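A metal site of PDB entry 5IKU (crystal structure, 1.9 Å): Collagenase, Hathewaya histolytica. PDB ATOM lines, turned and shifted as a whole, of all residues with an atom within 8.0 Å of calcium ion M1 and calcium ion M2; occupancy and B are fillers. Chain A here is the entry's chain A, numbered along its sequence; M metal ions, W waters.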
ATOM      1  N   GLU A  12      -0.670   6.526   6.722  1.00  0.00           N
ATOM      2  CA  GLU A  12      -0.321   7.832   6.157  1.00  0.00           C
ATOM      3  C   GLU A  12       1.102   7.804   5.608  1.00  0.00           C
ATOM      4  O   GLU A  12       1.901   6.937   5.966  1.00  0.00           O
ATOM      5  CB  GLU A  12      -0.482   8.944   7.214  1.00  0.00           C
ATOM      6  CG  GLU A  12       0.476   8.799   8.361  1.00  0.00           C
ATOM      7  CD  GLU A  12       0.535  10.059   9.181  1.00  0.00           C
ATOM      8  OE1 GLU A  12       0.357  11.170   8.620  1.00  0.00           O
ATOM      9  OE2 GLU A  12       0.821   9.931  10.390  1.00  0.00           O
ATOM     10  N   MET A  13       1.433   8.760   4.749  1.00  0.00           N
ATOM     11  CA  MET A  13       2.781   8.886   4.221  1.00  0.00           C
ATOM     12  C   MET A  13       3.122  10.384   4.198  1.00  0.00           C
ATOM     13  O   MET A  13       2.564  11.143   3.421  1.00  0.00           O
ATOM     14  CB  MET A  13       2.788   8.194   2.830  1.00  0.00           C
ATOM     15  CG  MET A  13       3.977   8.405   1.910  1.00  0.00           C
ATOM     16  SD  MET A  13       3.909   7.156   0.611  1.00  0.00           S
ATOM     17  CE  MET A  13       3.882   5.637   1.590  1.00  0.00           C
ATOM     18  N   GLU A  14       4.023  10.836   5.069  1.00  0.00           N
ATOM     19  CA  GLU A  14       4.385  12.248   5.138  1.00  0.00           C
ATOM     20  C   GLU A  14       5.244  12.638   3.920  1.00  0.00           C
ATOM     21  O   GLU A  14       5.939  11.783   3.390  1.00  0.00           O
ATOM     22  CB  GLU A  14       5.158  12.506   6.460  1.00  0.00           C
ATOM     23  CG  GLU A  14       4.259  12.275   7.690  1.00  0.00           C
ATOM     24  CD  GLU A  14       3.275  13.411   7.936  1.00  0.00           C
ATOM     25  OE1 GLU A  14       3.376  14.463   7.248  1.00  0.00           O
ATOM     26  OE2 GLU A  14       2.395  13.280   8.841  1.00  0.00           O
ATOM     27  N   PRO A  15       5.229  13.881   3.454  1.00  0.00           N
ATOM     28  CA  PRO A  15       4.421  14.956   3.996  1.00  0.00           C
ATOM     29  C   PRO A  15       3.001  14.894   3.453  1.00  0.00           C
ATOM     30  O   PRO A  15       2.788  14.567   2.295  1.00  0.00           O
ATOM     31  CB  PRO A  15       5.120  16.224   3.459  1.00  0.00           C
ATOM     32  CG  PRO A  15       5.666  15.773   2.144  1.00  0.00           C
ATOM     33  CD  PRO A  15       6.085  14.337   2.338  1.00  0.00           C
ATOM     34  N   ASN A  16       2.021  15.182   4.297  1.00  0.00           N
ATOM     35  CA  ASN A  16       0.622  15.189   3.808  1.00  0.00           C
ATOM     36  C   ASN A  16      -0.116  16.390   4.462  1.00  0.00           C
ATOM     37  O   ASN A  16      -1.252  16.294   4.843  1.00  0.00           O
ATOM     38  CB  ASN A  16      -0.036  13.872   4.208  1.00  0.00           C
ATOM     39  CG  ASN A  16       0.087  13.617   5.661  1.00  0.00           C
ATOM     40  OD1 ASN A  16       0.463  14.524   6.396  1.00  0.00           O
ATOM     41  ND2 ASN A  16      -0.188  12.375   6.107  1.00  0.00           N
ATOM     42  N   ASP A  17       0.566  17.548   4.560  1.00  0.00           N
ATOM     43  CA  ASP A  17       0.179  18.612   5.494  1.00  0.00           C
ATOM     44  C   ASP A  17      -0.905  19.615   5.016  1.00  0.00           C
ATOM     45  O   ASP A  17      -1.370  20.460   5.777  1.00  0.00           O
ATOM     46  CB  ASP A  17       1.409  19.347   6.020  1.00  0.00           C
ATOM     47  CG  ASP A  17       2.293  18.470   6.905  1.00  0.00           C
ATOM     48  OD1 ASP A  17       3.369  18.995   7.230  1.00  0.00           O
ATOM     49  OD2 ASP A  17       1.937  17.307   7.281  1.00  0.00           O
ATOM     50  N   ASP A  18      -1.294  19.506   3.746  1.00  0.00           N
ATOM     51  CA  ASP A  18      -2.354  20.331   3.186  1.00  0.00           C
ATOM     52  C   ASP A  18      -3.016  19.595   2.048  1.00  0.00           C
ATOM     53  O   ASP A  18      -2.606  18.466   1.704  1.00  0.00           O
ATOM     54  CB  ASP A  18      -1.839  21.721   2.736  1.00  0.00           C
ATOM     55  CG  ASP A  18      -0.914  21.653   1.521  1.00  0.00           C
ATOM     56  OD1 ASP A  18      -0.297  22.681   1.193  1.00  0.00           O
ATOM     57  OD2 ASP A  18      -0.787  20.591   0.886  1.00  0.00           O
ATOM     58  N   GLU A  21      -1.103  17.990  -0.958  1.00  0.00           N
ATOM     59  CA  GLU A  21      -0.344  16.739  -0.771  1.00  0.00           C
ATOM     60  C   GLU A  21      -1.125  15.713   0.066  1.00  0.00           C
ATOM     61  O   GLU A  21      -0.517  14.870   0.725  1.00  0.00           O
ATOM     62  CB  GLU A  21       1.063  16.996  -0.206  1.00  0.00           C
ATOM     63  CG  GLU A  21       1.102  18.126   0.798  1.00  0.00           C
ATOM     64  CD  GLU A  21       2.519  18.539   1.211  1.00  0.00           C
ATOM     65  OE1 GLU A  21       3.391  18.677   0.323  1.00  0.00           O
ATOM     66  OE2 GLU A  21       2.712  18.728   2.450  1.00  0.00           O
ATOM     67  N   ASN A  23      -2.856  12.433   1.432  1.00  0.00           N
ATOM     68  CA  ASN A  23      -2.699  10.994   1.103  1.00  0.00           C
ATOM     69  C   ASN A  23      -4.079  10.412   0.704  1.00  0.00           C
ATOM     70  O   ASN A  23      -5.105  10.798   1.252  1.00  0.00           O
ATOM     71  CB  ASN A  23      -2.193  10.205   2.291  1.00  0.00           C
ATOM     72  CG  ASN A  23      -0.835  10.674   2.819  1.00  0.00           C
ATOM     73  OD1 ASN A  23      -0.605  10.605   4.014  1.00  0.00           O
ATOM     74  ND2 ASN A  23       0.075  11.106   1.938  1.00  0.00           N
ATOM     75  N   LYS A  33      -4.066   4.316   9.649  1.00  0.00           N
ATOM     76  CA  LYS A  33      -3.422   4.740  10.891  1.00  0.00           C
ATOM     77  C   LYS A  33      -2.515   5.900  10.612  1.00  0.00           C
ATOM     78  O   LYS A  33      -1.930   5.995   9.534  1.00  0.00           O
ATOM     79  CB  LYS A  33      -2.561   3.639  11.501  1.00  0.00           C
ATOM     80  CG  LYS A  33      -3.332   2.447  12.021  1.00  0.00           C
ATOM     81  CD  LYS A  33      -2.444   1.566  12.898  1.00  0.00           C
ATOM     82  CE  LYS A  33      -3.214   0.338  13.351  1.00  0.00           C
ATOM     83  NZ  LYS A  33      -4.622   0.703  13.691  1.00  0.00           N
ATOM     84  N   GLY A  34      -2.395   6.791  11.585  1.00  0.00           N
ATOM     85  CA  GLY A  34      -1.371   7.815  11.534  1.00  0.00           C
ATOM     86  C   GLY A  34      -1.153   8.452  12.900  1.00  0.00           C
ATOM     87  O   GLY A  34      -1.716   8.028  13.896  1.00  0.00           O
ATOM     88  N   ASP A  35      -0.343   9.498  12.963  1.00  0.00           N
ATOM     89  CA  ASP A  35      -0.189  10.179  14.247  1.00  0.00           C
ATOM     90  C   ASP A  35       0.208  11.612  13.983  1.00  0.00           C
ATOM     91  O   ASP A  35       0.686  11.928  12.896  1.00  0.00           O
ATOM     92  CB  ASP A  35       0.849   9.495  15.128  1.00  0.00           C
ATOM     93  CG  ASP A  35       2.119   9.161  14.370  1.00  0.00           C
ATOM     94  OD1 ASP A  35       2.784  10.097  13.866  1.00  0.00           O
ATOM     95  OD2 ASP A  35       2.431   7.966  14.263  1.00  0.00           O
ATOM     96  N   LEU A  36      -0.003  12.467  14.977  1.00  0.00           N
ATOM     97  CA  LEU A  36       0.395  13.871  14.902  1.00  0.00           C
ATOM     98  C   LEU A  36       1.331  14.099  16.102  1.00  0.00           C
ATOM     99  O   LEU A  36       0.922  14.687  17.096  1.00  0.00           O
ATOM    100  CB  LEU A  36      -0.822  14.787  15.078  1.00  0.00           C
ATOM    101  CG  LEU A  36      -1.835  14.664  13.941  1.00  0.00           C
ATOM    102  CD1 LEU A  36      -3.117  15.327  14.445  1.00  0.00           C
ATOM    103  CD2 LEU A  36      -1.288  15.417  12.737  1.00  0.00           C
ATOM    104  N   ASN A  37       2.553  13.616  15.991  1.00  0.00           N
ATOM    105  CA  ASN A  37       3.475  13.640  17.123  1.00  0.00           C
ATOM    106  C   ASN A  37       4.437  14.818  16.935  1.00  0.00           C
ATOM    107  O   ASN A  37       4.846  15.098  15.794  1.00  0.00           O
ATOM    108  CB  ASN A  37       4.279  12.323  17.182  1.00  0.00           C
ATOM    109  CG  ASN A  37       3.447  11.133  17.672  1.00  0.00           C
ATOM    110  OD1 ASN A  37       2.461  11.278  18.405  1.00  0.00           O
ATOM    111  ND2 ASN A  37       3.864   9.951  17.270  1.00  0.00           N
ATOM    112  N   SER A  39       6.105  18.241  16.176  1.00  0.00           N
ATOM    113  CA  SER A  39       5.741  19.379  15.328  1.00  0.00           C
ATOM    114  C   SER A  39       4.963  18.965  14.065  1.00  0.00           C
ATOM    115  O   SER A  39       4.686  19.819  13.230  1.00  0.00           O
ATOM    116  CB  SER A  39       7.002  20.119  14.902  1.00  0.00           C
ATOM    117  OG  SER A  39       7.685  19.337  13.925  1.00  0.00           O
ATOM    118  N   ASP A  40       4.637  17.687  13.901  1.00  0.00           N
ATOM    119  CA  ASP A  40       3.703  17.326  12.779  1.00  0.00           C
ATOM    120  C   ASP A  40       2.294  17.704  13.254  1.00  0.00           C
ATOM    121  O   ASP A  40       1.701  16.998  14.089  1.00  0.00           O
ATOM    122  CB  ASP A  40       3.816  15.843  12.435  1.00  0.00           C
ATOM    123  CG  ASP A  40       2.770  15.398  11.434  1.00  0.00           C
ATOM    124  OD1 ASP A  40       2.478  16.155  10.489  1.00  0.00           O
ATOM    125  OD2 ASP A  40       2.218  14.285  11.591  1.00  0.00           O
ATOM    126  N   ASP A  41       1.752  18.826  12.798  1.00  0.00           N
ATOM    127  CA  ASP A  41       0.475  19.254  13.364  1.00  0.00           C
ATOM    128  C   ASP A  41      -0.722  19.165  12.455  1.00  0.00           C
ATOM    129  O   ASP A  41      -1.839  19.562  12.873  1.00  0.00           O
ATOM    130  CB  ASP A  41       0.549  20.642  14.022  1.00  0.00           C
ATOM    131  CG  ASP A  41       0.911  21.726  13.057  1.00  0.00           C
ATOM    132  OD1 ASP A  41       1.150  21.390  11.881  1.00  0.00           O
ATOM    133  OD2 ASP A  41       0.967  22.909  13.472  1.00  0.00           O
ATOM    134  N   ALA A  42      -0.514  18.683  11.217  1.00  0.00           N
ATOM    135  CA  ALA A  42      -1.658  18.495  10.314  1.00  0.00           C
ATOM    136  C   ALA A  42      -1.418  17.318   9.356  1.00  0.00           C
ATOM    137  O   ALA A  42      -0.319  17.136   8.867  1.00  0.00           O
ATOM    138  CB  ALA A  42      -1.878  19.766   9.505  1.00  0.00           C
ATOM    139  N   ASP A  43      -2.466  16.529   9.137  1.00  0.00           N
ATOM    140  CA  ASP A  43      -2.455  15.380   8.223  1.00  0.00           C
ATOM    141  C   ASP A  43      -3.722  15.536   7.372  1.00  0.00           C
ATOM    142  O   ASP A  43      -4.792  15.810   7.932  1.00  0.00           O
ATOM    143  CB  ASP A  43      -2.569  14.042   8.996  1.00  0.00           C
ATOM    144  CG  ASP A  43      -1.286  13.674   9.726  1.00  0.00           C
ATOM    145  OD1 ASP A  43      -0.257  14.342   9.466  1.00  0.00           O
ATOM    146  OD2 ASP A  43      -1.291  12.711  10.530  1.00  0.00           O
ATOM    147  N   THR A  44      -3.596  15.279   6.076  1.00  0.00           N
ATOM    148  CA  THR A  44      -4.680  15.453   5.117  1.00  0.00           C
ATOM    149  C   THR A  44      -4.824  14.213   4.248  1.00  0.00           C
ATOM    150  O   THR A  44      -3.809  13.645   3.779  1.00  0.00           O
ATOM    151  CB  THR A  44      -4.434  16.693   4.200  1.00  0.00           C
ATOM    152  OG1 THR A  44      -3.859  17.732   4.988  1.00  0.00           O
ATOM    153  CG2 THR A  44      -5.749  17.161   3.543  1.00  0.00           C
ATOM    154  N   PHE A  45      -6.086  13.768   4.086  1.00  0.00           N
ATOM    155  CA  PHE A  45      -6.422  12.599   3.298  1.00  0.00           C
ATOM    156  C   PHE A  45      -7.547  12.951   2.366  1.00  0.00           C
ATOM    157  O   PHE A  45      -8.309  13.862   2.619  1.00  0.00           O
ATOM    158  CB  PHE A  45      -6.938  11.476   4.229  1.00  0.00           C
ATOM    159  CG  PHE A  45      -5.932  11.076   5.288  1.00  0.00           C
ATOM    160  CD1 PHE A  45      -5.937  11.682   6.538  1.00  0.00           C
ATOM    161  CD2 PHE A  45      -4.944  10.116   4.997  1.00  0.00           C
ATOM    162  CE1 PHE A  45      -4.986  11.343   7.500  1.00  0.00           C
ATOM    163  CE2 PHE A  45      -3.983   9.782   5.962  1.00  0.00           C
ATOM    164  CZ  PHE A  45      -4.017  10.395   7.219  1.00  0.00           C
ATOM    165  N   ILE A 106      -6.856  16.819   9.481  1.00  0.00           N
ATOM    166  CA  ILE A 106      -6.799  16.559  10.893  1.00  0.00           C
ATOM    167  C   ILE A 106      -5.659  17.439  11.389  1.00  0.00           C
ATOM    168  O   ILE A 106      -4.582  17.378  10.830  1.00  0.00           O
ATOM    169  CB  ILE A 106      -6.471  15.090  11.139  1.00  0.00           C
ATOM    170  CG1 ILE A 106      -7.466  14.193  10.447  1.00  0.00           C
ATOM    171  CG2 ILE A 106      -6.501  14.785  12.645  1.00  0.00           C
ATOM    172  CD1 ILE A 106      -6.990  12.767  10.323  1.00  0.00           C
ATOM    173  N   ILE A 115      -0.429  12.613  19.539  1.00  0.00           N
ATOM    174  CA  ILE A 115      -1.738  12.057  19.281  1.00  0.00           C
ATOM    175  C   ILE A 115      -1.530  10.936  18.272  1.00  0.00           C
ATOM    176  O   ILE A 115      -0.877  11.136  17.267  1.00  0.00           O
ATOM    177  CB  ILE A 115      -2.677  13.133  18.666  1.00  0.00           C
ATOM    178  CG1 ILE A 115      -2.811  14.328  19.621  1.00  0.00           C
ATOM    179  CG2 ILE A 115      -4.039  12.545  18.289  1.00  0.00           C
ATOM    180  CD1 ILE A 115      -3.146  15.593  18.865  1.00  0.00           C
ATOM    181  N   TYR A 117      -3.946   8.063  15.965  1.00  0.00           N
ATOM    182  CA  TYR A 117      -5.337   7.922  15.632  1.00  0.00           C
ATOM    183  C   TYR A 117      -5.480   6.835  14.609  1.00  0.00           C
ATOM    184  O   TYR A 117      -4.507   6.418  13.942  1.00  0.00           O
ATOM    185  CB  TYR A 117      -5.894   9.228  15.025  1.00  0.00           C
ATOM    186  CG  TYR A 117      -5.168   9.706  13.780  1.00  0.00           C
ATOM    187  CD1 TYR A 117      -5.460   9.146  12.512  1.00  0.00           C
ATOM    188  CD2 TYR A 117      -4.170  10.693  13.872  1.00  0.00           C
ATOM    189  CE1 TYR A 117      -4.796   9.561  11.379  1.00  0.00           C
ATOM    190  CE2 TYR A 117      -3.503  11.129  12.733  1.00  0.00           C
ATOM    191  CZ  TYR A 117      -3.820  10.555  11.494  1.00  0.00           C
ATOM    192  OH  TYR A 117      -3.170  10.934  10.346  1.00  0.00           O
HETATM  193 CA    CA M   1       1.430  15.550   8.398  1.00  0.00          CA
HETATM  194 CA    CA M   2       1.136  12.434  10.556  1.00  0.00          CA
HETATM  195  O   HOH W   1       3.285  11.327  11.344  1.00  0.00           O
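The backbone NH (N) of Asp 17 is in hydrogen-bond range of the side-chain carboxylate (OE2) of Glu 21 (3.2 Å).
OD2 of Asp 43 sits close to OH of Tyr 117, at 2.6 Å.
The backbone carbonyl oxygen of Asp 43 is in hydrogen-bond range of the backbone NH of Ile 106, at 2.8 Å.
The side-chain carboxylate of Glu 12 lies close to the side-chain amide nitrogen of Asn 16 (2.8 Å).
The backbone carbonyl oxygen of Lys 33 sits at hydrogen-bond distance from the backbone NH of Glu 12 (3.1 Å).
The backbone carbonyl oxygen of Asn 16 sits at hydrogen-bond distance from the backbone NH of Thr 44, 2.8 Å away.
OD1 of Asn 23 lies within hydrogen-bond range of ND2 of Asn 16, at 2.8 Å.
Of the 24 residues printed, 6 come within 4 Å of calcium ion M1.
Of the 24 residues printed, 5 come within 4 Å of calcium ion M2.
The nearest printed residue that does not touch calcium ion M2 is Leu 36 (4.4 Å).
Calcium ion M1 is bound by the side-chain carboxylate (OD2) of Asp 17, the side-chain carboxylate (OD1) of Asp 43, the backbone carbonyl oxygen (O) of Ala 42, the side-chain carboxylate (OD1) of Asp 40, the side-chain amide oxygen (OD1) of Asn 16, the side-chain carboxylate (OE2) of Glu 14 and the side-chain carboxylate (OE1) of Glu 14.
Calcium ion M1 has seven donor atoms within binding distance.
Calcium ion M2 is bound by the side-chain carboxylate (OE2) of Glu 14, the side-chain carboxylate (OD2) of Asp 40, the backbone carbonyl oxygen (O) of Asp 35, the side-chain carboxylate (OE1) of Glu 12, the side-chain carboxylate (OD2) of Asp 43, the side-chain carboxylate (OE2) of Glu 12, water W1 and the side-chain carboxylate (OD1) of Asp 43.
Calcium ion M2 has eight donor atoms within binding distance.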
